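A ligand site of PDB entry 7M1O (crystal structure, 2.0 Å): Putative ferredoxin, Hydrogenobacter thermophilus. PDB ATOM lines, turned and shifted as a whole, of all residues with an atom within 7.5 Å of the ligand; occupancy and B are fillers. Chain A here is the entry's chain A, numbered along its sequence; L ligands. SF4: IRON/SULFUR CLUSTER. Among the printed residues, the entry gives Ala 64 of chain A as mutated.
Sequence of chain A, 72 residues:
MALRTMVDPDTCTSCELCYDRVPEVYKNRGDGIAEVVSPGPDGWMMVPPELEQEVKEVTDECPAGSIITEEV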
ATOM      1  N   MET A   6      -6.401 -23.070  28.192  1.00  0.00           N
ATOM      2  CA  MET A   6      -5.221 -23.221  27.356  1.00  0.00           C
ATOM      3  C   MET A   6      -5.081 -22.020  26.438  1.00  0.00           C
ATOM      4  O   MET A   6      -6.034 -21.266  26.254  1.00  0.00           O
ATOM      5  CB  MET A   6      -5.281 -24.521  26.528  1.00  0.00           C
ATOM      6  CG  MET A   6      -6.381 -24.554  25.466  1.00  0.00           C
ATOM      7  SD  MET A   6      -6.045 -25.789  24.185  1.00  0.00           S
ATOM      8  CE  MET A   6      -7.570 -25.780  23.258  1.00  0.00           C
ATOM      9  N   VAL A   7      -3.897 -21.852  25.863  1.00  0.00           N
ATOM     10  CA  VAL A   7      -3.655 -20.801  24.877  1.00  0.00           C
ATOM     11  C   VAL A   7      -3.306 -21.422  23.525  1.00  0.00           C
ATOM     12  O   VAL A   7      -2.459 -22.306  23.446  1.00  0.00           O
ATOM     13  CB  VAL A   7      -2.508 -19.861  25.310  1.00  0.00           C
ATOM     14  CG1 VAL A   7      -2.197 -18.838  24.219  1.00  0.00           C
ATOM     15  CG2 VAL A   7      -2.879 -19.150  26.608  1.00  0.00           C
ATOM     16  N   ASP A   8      -3.984 -20.952  22.484  1.00  0.00           N
ATOM     17  CA  ASP A   8      -3.688 -21.376  21.127  1.00  0.00           C
ATOM     18  C   ASP A   8      -2.591 -20.475  20.543  1.00  0.00           C
ATOM     19  O   ASP A   8      -2.881 -19.354  20.140  1.00  0.00           O
ATOM     20  CB  ASP A   8      -4.946 -21.320  20.252  1.00  0.00           C
ATOM     21  CG  ASP A   8      -4.766 -21.993  18.908  1.00  0.00           C
ATOM     22  OD1 ASP A   8      -3.606 -22.201  18.497  1.00  0.00           O
ATOM     23  OD2 ASP A   8      -5.779 -22.314  18.270  1.00  0.00           O
ATOM     24  N   PRO A   9      -1.340 -20.958  20.499  1.00  0.00           N
ATOM     25  CA  PRO A   9      -0.252 -20.084  20.069  1.00  0.00           C
ATOM     26  C   PRO A   9      -0.347 -19.692  18.602  1.00  0.00           C
ATOM     27  O   PRO A   9       0.256 -18.700  18.191  1.00  0.00           O
ATOM     28  CB  PRO A   9       0.998 -20.939  20.318  1.00  0.00           C
ATOM     29  CG  PRO A   9       0.516 -22.335  20.152  1.00  0.00           C
ATOM     30  CD  PRO A   9      -0.877 -22.342  20.703  1.00  0.00           C
ATOM     31  N   THR A  11      -2.766 -18.431  17.033  1.00  0.00           N
ATOM     32  CA  THR A  11      -3.596 -17.256  16.810  1.00  0.00           C
ATOM     33  C   THR A  11      -3.257 -16.083  17.744  1.00  0.00           C
ATOM     34  O   THR A  11      -3.700 -14.957  17.513  1.00  0.00           O
ATOM     35  CB  THR A  11      -5.092 -17.594  16.990  1.00  0.00           C
ATOM     36  OG1 THR A  11      -5.315 -18.086  18.312  1.00  0.00           O
ATOM     37  CG2 THR A  11      -5.518 -18.640  15.968  1.00  0.00           C
ATOM     38  N   CYS A  12      -2.490 -16.365  18.800  1.00  0.00           N
ATOM     39  CA  CYS A  12      -2.110 -15.325  19.761  1.00  0.00           C
ATOM     40  C   CYS A  12      -1.330 -14.198  19.083  1.00  0.00           C
ATOM     41  O   CYS A  12      -0.429 -14.454  18.292  1.00  0.00           O
ATOM     42  CB  CYS A  12      -1.263 -15.932  20.883  1.00  0.00           C
ATOM     43  SG  CYS A  12      -0.577 -14.707  22.018  1.00  0.00           S
ATOM     44  N   THR A  13      -1.693 -12.969  19.408  1.00  0.00           N
ATOM     45  CA  THR A  13      -1.091 -11.788  18.783  1.00  0.00           C
ATOM     46  C   THR A  13      -0.164 -11.050  19.736  1.00  0.00           C
ATOM     47  O   THR A  13       0.241  -9.911  19.458  1.00  0.00           O
ATOM     48  CB  THR A  13      -2.182 -10.831  18.267  1.00  0.00           C
ATOM     49  OG1 THR A  13      -3.032 -10.438  19.353  1.00  0.00           O
ATOM     50  CG2 THR A  13      -3.022 -11.504  17.196  1.00  0.00           C
ATOM     51  N   SER A  14       0.176 -11.690  20.849  1.00  0.00           N
ATOM     52  CA  SER A  14       1.155 -11.159  21.799  1.00  0.00           C
ATOM     53  C   SER A  14       0.738  -9.807  22.365  1.00  0.00           C
ATOM     54  O   SER A  14       1.573  -8.928  22.569  1.00  0.00           O
ATOM     55  CB  SER A  14       2.527 -11.042  21.127  1.00  0.00           C
ATOM     56  OG  SER A  14       2.955 -12.297  20.645  1.00  0.00           O
ATOM     57  N   CYS A  15      -0.556  -9.651  22.640  1.00  0.00           N
ATOM     58  CA  CYS A  15      -1.086  -8.388  23.135  1.00  0.00           C
ATOM     59  C   CYS A  15      -0.787  -8.174  24.623  1.00  0.00           C
ATOM     60  O   CYS A  15      -0.970  -7.081  25.152  1.00  0.00           O
ATOM     61  CB  CYS A  15      -2.588  -8.315  22.890  1.00  0.00           C
ATOM     62  SG  CYS A  15      -3.561  -9.118  24.158  1.00  0.00           S
ATOM     63  N   GLU A  16      -0.344  -9.241  25.282  1.00  0.00           N
ATOM     64  CA  GLU A  16       0.134  -9.213  26.670  1.00  0.00           C
ATOM     65  C   GLU A  16      -0.976  -9.098  27.727  1.00  0.00           C
ATOM     66  O   GLU A  16      -0.683  -8.986  28.912  1.00  0.00           O
ATOM     67  CB  GLU A  16       1.139  -8.064  26.876  1.00  0.00           C
ATOM     68  CG  GLU A  16       2.242  -7.995  25.827  1.00  0.00           C
ATOM     69  CD  GLU A  16       3.411  -7.105  26.243  1.00  0.00           C
ATOM     70  OE1 GLU A  16       3.449  -6.663  27.414  1.00  0.00           O
ATOM     71  OE2 GLU A  16       4.289  -6.851  25.399  1.00  0.00           O
ATOM     72  N   LEU A  17      -2.231  -9.131  27.309  1.00  0.00           N
ATOM     73  CA  LEU A  17      -3.330  -8.910  28.247  1.00  0.00           C
ATOM     74  C   LEU A  17      -3.427 -10.012  29.293  1.00  0.00           C
ATOM     75  O   LEU A  17      -3.480  -9.722  30.494  1.00  0.00           O
ATOM     76  CB  LEU A  17      -4.662  -8.802  27.506  1.00  0.00           C
ATOM     77  CG  LEU A  17      -5.890  -8.556  28.397  1.00  0.00           C
ATOM     78  CD1 LEU A  17      -5.774  -7.223  29.133  1.00  0.00           C
ATOM     79  CD2 LEU A  17      -7.170  -8.615  27.592  1.00  0.00           C
ATOM     80  N   CYS A  18      -3.445 -11.263  28.853  1.00  0.00           N
ATOM     81  CA  CYS A  18      -3.718 -12.370  29.773  1.00  0.00           C
ATOM     82  C   CYS A  18      -2.639 -12.544  30.839  1.00  0.00           C
ATOM     83  O   CYS A  18      -2.971 -12.738  32.012  1.00  0.00           O
ATOM     84  CB  CYS A  18      -3.899 -13.679  28.996  1.00  0.00           C
ATOM     85  SG  CYS A  18      -2.504 -14.130  27.949  1.00  0.00           S
ATOM     86  N   TYR A  19      -1.367 -12.466  30.449  1.00  0.00           N
ATOM     87  CA  TYR A  19      -0.319 -12.728  31.435  1.00  0.00           C
ATOM     88  C   TYR A  19       0.092 -11.471  32.199  1.00  0.00           C
ATOM     89  O   TYR A  19       0.821 -11.564  33.185  1.00  0.00           O
ATOM     90  CB  TYR A  19       0.916 -13.375  30.778  1.00  0.00           C
ATOM     91  CG  TYR A  19       1.497 -12.747  29.533  1.00  0.00           C
ATOM     92  CD1 TYR A  19       1.335 -13.372  28.292  1.00  0.00           C
ATOM     93  CD2 TYR A  19       2.265 -11.596  29.585  1.00  0.00           C
ATOM     94  CE1 TYR A  19       1.881 -12.834  27.157  1.00  0.00           C
ATOM     95  CE2 TYR A  19       2.817 -11.049  28.436  1.00  0.00           C
ATOM     96  CZ  TYR A  19       2.623 -11.683  27.226  1.00  0.00           C
ATOM     97  OH  TYR A  19       3.166 -11.158  26.073  1.00  0.00           O
ATOM     98  N   ASP A  20      -0.404 -10.311  31.775  1.00  0.00           N
ATOM     99  CA  ASP A  20      -0.302  -9.118  32.604  1.00  0.00           C
ATOM    100  C   ASP A  20      -1.392  -9.139  33.683  1.00  0.00           C
ATOM    101  O   ASP A  20      -1.149  -8.814  34.838  1.00  0.00           O
ATOM    102  CB  ASP A  20      -0.425  -7.848  31.777  1.00  0.00           C
ATOM    103  CG  ASP A  20      -0.315  -6.590  32.622  1.00  0.00           C
ATOM    104  OD1 ASP A  20       0.725  -6.433  33.298  1.00  0.00           O
ATOM    105  OD2 ASP A  20      -1.261  -5.790  32.647  1.00  0.00           O
ATOM    106  N   TYR A  26      -1.279 -17.291  33.292  1.00  0.00           N
ATOM    107  CA  TYR A  26      -0.612 -17.109  32.000  1.00  0.00           C
ATOM    108  C   TYR A  26       0.732 -16.424  32.132  1.00  0.00           C
ATOM    109  O   TYR A  26       0.948 -15.631  33.045  1.00  0.00           O
ATOM    110  CB  TYR A  26      -1.508 -16.307  31.050  1.00  0.00           C
ATOM    111  CG  TYR A  26      -2.920 -16.842  30.956  1.00  0.00           C
ATOM    112  CD1 TYR A  26      -3.225 -17.902  30.117  1.00  0.00           C
ATOM    113  CD2 TYR A  26      -3.942 -16.291  31.717  1.00  0.00           C
ATOM    114  CE1 TYR A  26      -4.515 -18.398  30.028  1.00  0.00           C
ATOM    115  CE2 TYR A  26      -5.230 -16.785  31.638  1.00  0.00           C
ATOM    116  CZ  TYR A  26      -5.508 -17.833  30.790  1.00  0.00           C
ATOM    117  OH  TYR A  26      -6.797 -18.317  30.710  1.00  0.00           O
ATOM    118  N   LYS A  27       1.634 -16.723  31.203  1.00  0.00           N
ATOM    119  CA  LYS A  27       2.948 -16.092  31.155  1.00  0.00           C
ATOM    120  C   LYS A  27       3.389 -15.884  29.723  1.00  0.00           C
ATOM    121  O   LYS A  27       2.946 -16.586  28.814  1.00  0.00           O
ATOM    122  CB  LYS A  27       3.984 -16.948  31.904  1.00  0.00           C
ATOM    123  CG  LYS A  27       4.327 -18.253  31.190  1.00  0.00           C
ATOM    124  CD  LYS A  27       5.244 -19.142  32.027  1.00  0.00           C
ATOM    125  CE  LYS A  27       5.543 -20.445  31.302  1.00  0.00           C
ATOM    126  NZ  LYS A  27       6.303 -21.417  32.140  1.00  0.00           N
ATOM    127  N   GLY A  32       6.749 -13.252  23.324  1.00  0.00           N
ATOM    128  CA  GLY A  32       5.543 -12.440  23.272  1.00  0.00           C
ATOM    129  C   GLY A  32       4.279 -13.269  23.316  1.00  0.00           C
ATOM    130  O   GLY A  32       3.261 -12.827  23.847  1.00  0.00           O
ATOM    131  N   ILE A  33       4.331 -14.478  22.757  1.00  0.00           N
ATOM    132  CA  ILE A  33       3.176 -15.370  22.756  1.00  0.00           C
ATOM    133  C   ILE A  33       2.916 -15.906  24.157  1.00  0.00           C
ATOM    134  O   ILE A  33       3.852 -16.226  24.888  1.00  0.00           O
ATOM    135  CB  ILE A  33       3.359 -16.566  21.786  1.00  0.00           C
ATOM    136  CG1 ILE A  33       3.595 -16.069  20.356  1.00  0.00           C
ATOM    137  CG2 ILE A  33       2.150 -17.498  21.837  1.00  0.00           C
ATOM    138  CD1 ILE A  33       2.400 -15.380  19.729  1.00  0.00           C
ATOM    139  N   ALA A  34       1.640 -15.987  24.528  1.00  0.00           N
ATOM    140  CA  ALA A  34       1.258 -16.451  25.850  1.00  0.00           C
ATOM    141  C   ALA A  34       1.172 -17.965  25.927  1.00  0.00           C
ATOM    142  O   ALA A  34       0.970 -18.639  24.915  1.00  0.00           O
ATOM    143  CB  ALA A  34      -0.071 -15.829  26.252  1.00  0.00           C
ATOM    144  N   GLU A  35       1.338 -18.492  27.132  1.00  0.00           N
ATOM    145  CA  GLU A  35       1.078 -19.905  27.420  1.00  0.00           C
ATOM    146  C   GLU A  35       0.685 -20.021  28.875  1.00  0.00           C
ATOM    147  O   GLU A  35       1.048 -19.181  29.691  1.00  0.00           O
ATOM    148  CB  GLU A  35       2.310 -20.771  27.110  1.00  0.00           C
ATOM    149  CG  GLU A  35       3.535 -20.446  27.969  1.00  0.00           C
ATOM    150  CD  GLU A  35       4.719 -21.350  27.657  1.00  0.00           C
ATOM    151  OE1 GLU A  35       5.809 -21.106  28.199  1.00  0.00           O
ATOM    152  OE2 GLU A  35       4.543 -22.311  26.873  1.00  0.00           O
ATOM    153  N   VAL A  58     -10.611 -12.751  30.979  1.00  0.00           N
ATOM    154  CA  VAL A  58      -9.571 -12.583  29.967  1.00  0.00           C
ATOM    155  C   VAL A  58      -9.847 -13.455  28.750  1.00  0.00           C
ATOM    156  O   VAL A  58      -9.415 -13.143  27.644  1.00  0.00           O
ATOM    157  CB  VAL A  58      -8.165 -12.908  30.504  1.00  0.00           C
ATOM    158  CG1 VAL A  58      -7.792 -11.963  31.642  1.00  0.00           C
ATOM    159  CG2 VAL A  58      -8.079 -14.357  30.956  1.00  0.00           C
ATOM    160  N   THR A  59     -10.554 -14.556  28.956  1.00  0.00           N
ATOM    161  CA  THR A  59     -10.965 -15.417  27.862  1.00  0.00           C
ATOM    162  C   THR A  59     -11.879 -14.660  26.905  1.00  0.00           C
ATOM    163  O   THR A  59     -11.755 -14.779  25.685  1.00  0.00           O
ATOM    164  CB  THR A  59     -11.678 -16.682  28.385  1.00  0.00           C
ATOM    165  OG1 THR A  59     -10.782 -17.458  29.183  1.00  0.00           O
ATOM    166  CG2 THR A  59     -12.178 -17.546  27.229  1.00  0.00           C
ATOM    167  N   GLU A  61     -11.936 -11.419  26.751  1.00  0.00           N
ATOM    168  CA  GLU A  61     -11.249 -10.181  26.398  1.00  0.00           C
ATOM    169  C   GLU A  61     -10.085 -10.397  25.432  1.00  0.00           C
ATOM    170  O   GLU A  61      -9.643  -9.446  24.784  1.00  0.00           O
ATOM    171  CB  GLU A  61     -10.747  -9.484  27.659  1.00  0.00           C
ATOM    172  CG  GLU A  61     -11.850  -8.861  28.498  1.00  0.00           C
ATOM    173  CD  GLU A  61     -11.373  -8.398  29.853  1.00  0.00           C
ATOM    174  OE1 GLU A  61     -10.228  -8.705  30.229  1.00  0.00           O
ATOM    175  OE2 GLU A  61     -12.155  -7.711  30.552  1.00  0.00           O
ATOM    176  N   CYS A  62      -9.604 -11.623  25.329  1.00  0.00           N
ATOM    177  CA  CYS A  62      -8.541 -11.934  24.374  1.00  0.00           C
ATOM    178  C   CYS A  62      -8.964 -11.505  22.978  1.00  0.00           C
ATOM    179  O   CYS A  62      -9.982 -11.980  22.465  1.00  0.00           O
ATOM    180  CB  CYS A  62      -8.209 -13.429  24.391  1.00  0.00           C
ATOM    181  SG  CYS A  62      -7.037 -13.931  23.103  1.00  0.00           S
ATOM    182  N   PRO A  63      -8.181 -10.606  22.343  1.00  0.00           N
ATOM    183  CA  PRO A  63      -8.591 -10.058  21.045  1.00  0.00           C
ATOM    184  C   PRO A  63      -8.592 -11.082  19.908  1.00  0.00           C
ATOM    185  O   PRO A  63      -9.265 -10.871  18.906  1.00  0.00           O
ATOM    186  CB  PRO A  63      -7.531  -8.975  20.791  1.00  0.00           C
ATOM    187  CG  PRO A  63      -6.332  -9.442  21.519  1.00  0.00           C
ATOM    188  CD  PRO A  63      -6.860 -10.104  22.758  1.00  0.00           C
ATOM    189  N   ALA A  64      -7.845 -12.175  20.082  1.00  0.00           N
ATOM    190  CA  ALA A  64      -7.660 -13.152  19.006  1.00  0.00           C
ATOM    191  C   ALA A  64      -8.445 -14.444  19.237  1.00  0.00           C
ATOM    192  O   ALA A  64      -8.411 -15.353  18.403  1.00  0.00           O
ATOM    193  CB  ALA A  64      -6.189 -13.461  18.833  1.00  0.00           C
ATOM    194  N   GLY A  65      -9.140 -14.533  20.371  1.00  0.00           N
ATOM    195  CA  GLY A  65      -9.877 -15.742  20.700  1.00  0.00           C
ATOM    196  C   GLY A  65      -8.942 -16.924  20.847  1.00  0.00           C
ATOM    197  O   GLY A  65      -9.310 -18.060  20.540  1.00  0.00           O
ATOM    198  N   SER A  66      -7.742 -16.651  21.346  1.00  0.00           N
ATOM    199  CA  SER A  66      -6.697 -17.670  21.456  1.00  0.00           C
ATOM    200  C   SER A  66      -6.827 -18.474  22.733  1.00  0.00           C
ATOM    201  O   SER A  66      -6.371 -19.614  22.807  1.00  0.00           O
ATOM    202  CB  SER A  66      -5.314 -17.010  21.406  1.00  0.00           C
ATOM    203  OG  SER A  66      -5.146 -16.259  20.214  1.00  0.00           O
ATOM    204  N   ILE A  67      -7.438 -17.875  23.743  1.00  0.00           N
ATOM    205  CA  ILE A  67      -7.612 -18.540  25.024  1.00  0.00           C
ATOM    206  C   ILE A  67      -8.865 -19.396  25.019  1.00  0.00           C
ATOM    207  O   ILE A  67      -9.982 -18.884  24.869  1.00  0.00           O
ATOM    208  CB  ILE A  67      -7.676 -17.532  26.181  1.00  0.00           C
ATOM    209  CG1 ILE A  67      -6.441 -16.641  26.173  1.00  0.00           C
ATOM    210  CG2 ILE A  67      -7.797 -18.274  27.517  1.00  0.00           C
ATOM    211  CD1 ILE A  67      -6.425 -15.567  27.224  1.00  0.00           C
HETATM  212 FE1  SF4 L   1      -2.248 -13.719  23.213  1.00  0.00          FE
HETATM  213 FE2  SF4 L   1      -4.909 -13.524  23.795  1.00  0.00          FE
HETATM  214 FE3  SF4 L   1      -3.271 -11.369  24.155  1.00  0.00          FE
HETATM  215 FE4  SF4 L   1      -3.050 -13.533  25.815  1.00  0.00          FE
HETATM  216  S1  SF4 L   1      -4.841 -12.144  25.611  1.00  0.00           S
HETATM  217  S2  SF4 L   1      -1.345 -12.385  24.830  1.00  0.00           S
HETATM  218  S3  SF4 L   1      -3.511 -15.226  24.364  1.00  0.00           S
HETATM  219  S4  SF4 L   1      -3.768 -12.385  22.181  1.00  0.00           S
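Merely in contact with the ligand: Val 7 (3.8 Å), Ser 14 (3.9 Å), Leu 17 (3.8 Å), Ala 34 (3.8 Å), Pro 63 (3.9 Å), Ser 66 (3.9 Å) and Ile 67 (3.7 Å).
13 residues have an atom within 4 Å of the ligand: Val 7, Cys 12, Thr 13, Ser 14, Cys 15, Glu 16, Leu 17, Cys 18, Ala 34, Cys 62, Pro 63, Ser 66 and Ile 67.
The side-chain sulfur of Cys 15 lies close to the backbone NH of Leu 17.
The side-chain sulfur of Cys 62 sits close to the backbone NH of Gly 65, 3.5 Å away.
N of Asp 8 sits at hydrogen-bond distance from O of Ser 66 (2.8 Å).
The side-chain hydroxyl (OG) of Ser 66 lies within hydrogen-bond range of the side-chain hydroxyl (OG1) of Thr 11, 2.6 Å away.
SG of Cys 12 sits close to N of Ser 14, at 3.3 Å.
The side-chain sulfur (SG) of Cys 62 lies close to the backbone NH (N) of Ser 66, at 3.3 Å.
SG of Cys 62 lies close to N of Ala 64.
SG of Cys 12 lies close to N of Ala 34 (3.6 Å).
OG1 of Thr 13 sits close to S4 of the ligand, at 3.5 Å.
A sulfur (S2) of the ligand sits close to the backbone NH (N) of Cys 15 (3.6 Å).
An iron atom (FE1) of the ligand is bound by the side-chain sulfur (SG) of Cys 12.
A sulfur (S1) of the ligand lies close to the backbone NH (N) of Cys 18 (3.6 Å).
A sulfur (S2) of the ligand sits close to the backbone NH of Glu 16, at 3.3 Å.
The backbone NH of Thr 13 sits close to a sulfur (S4) of the ligand (3.5 Å).
An iron atom (FE3) of the ligand is bound by the side-chain sulfur of Cys 15 (2.3 Å).
SG of Cys 18 binds FE4 of the ligand, at 2.3 Å.
The side-chain sulfur (SG) of Cys 62 binds an iron atom (FE2) of the ligand (2.3 Å).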
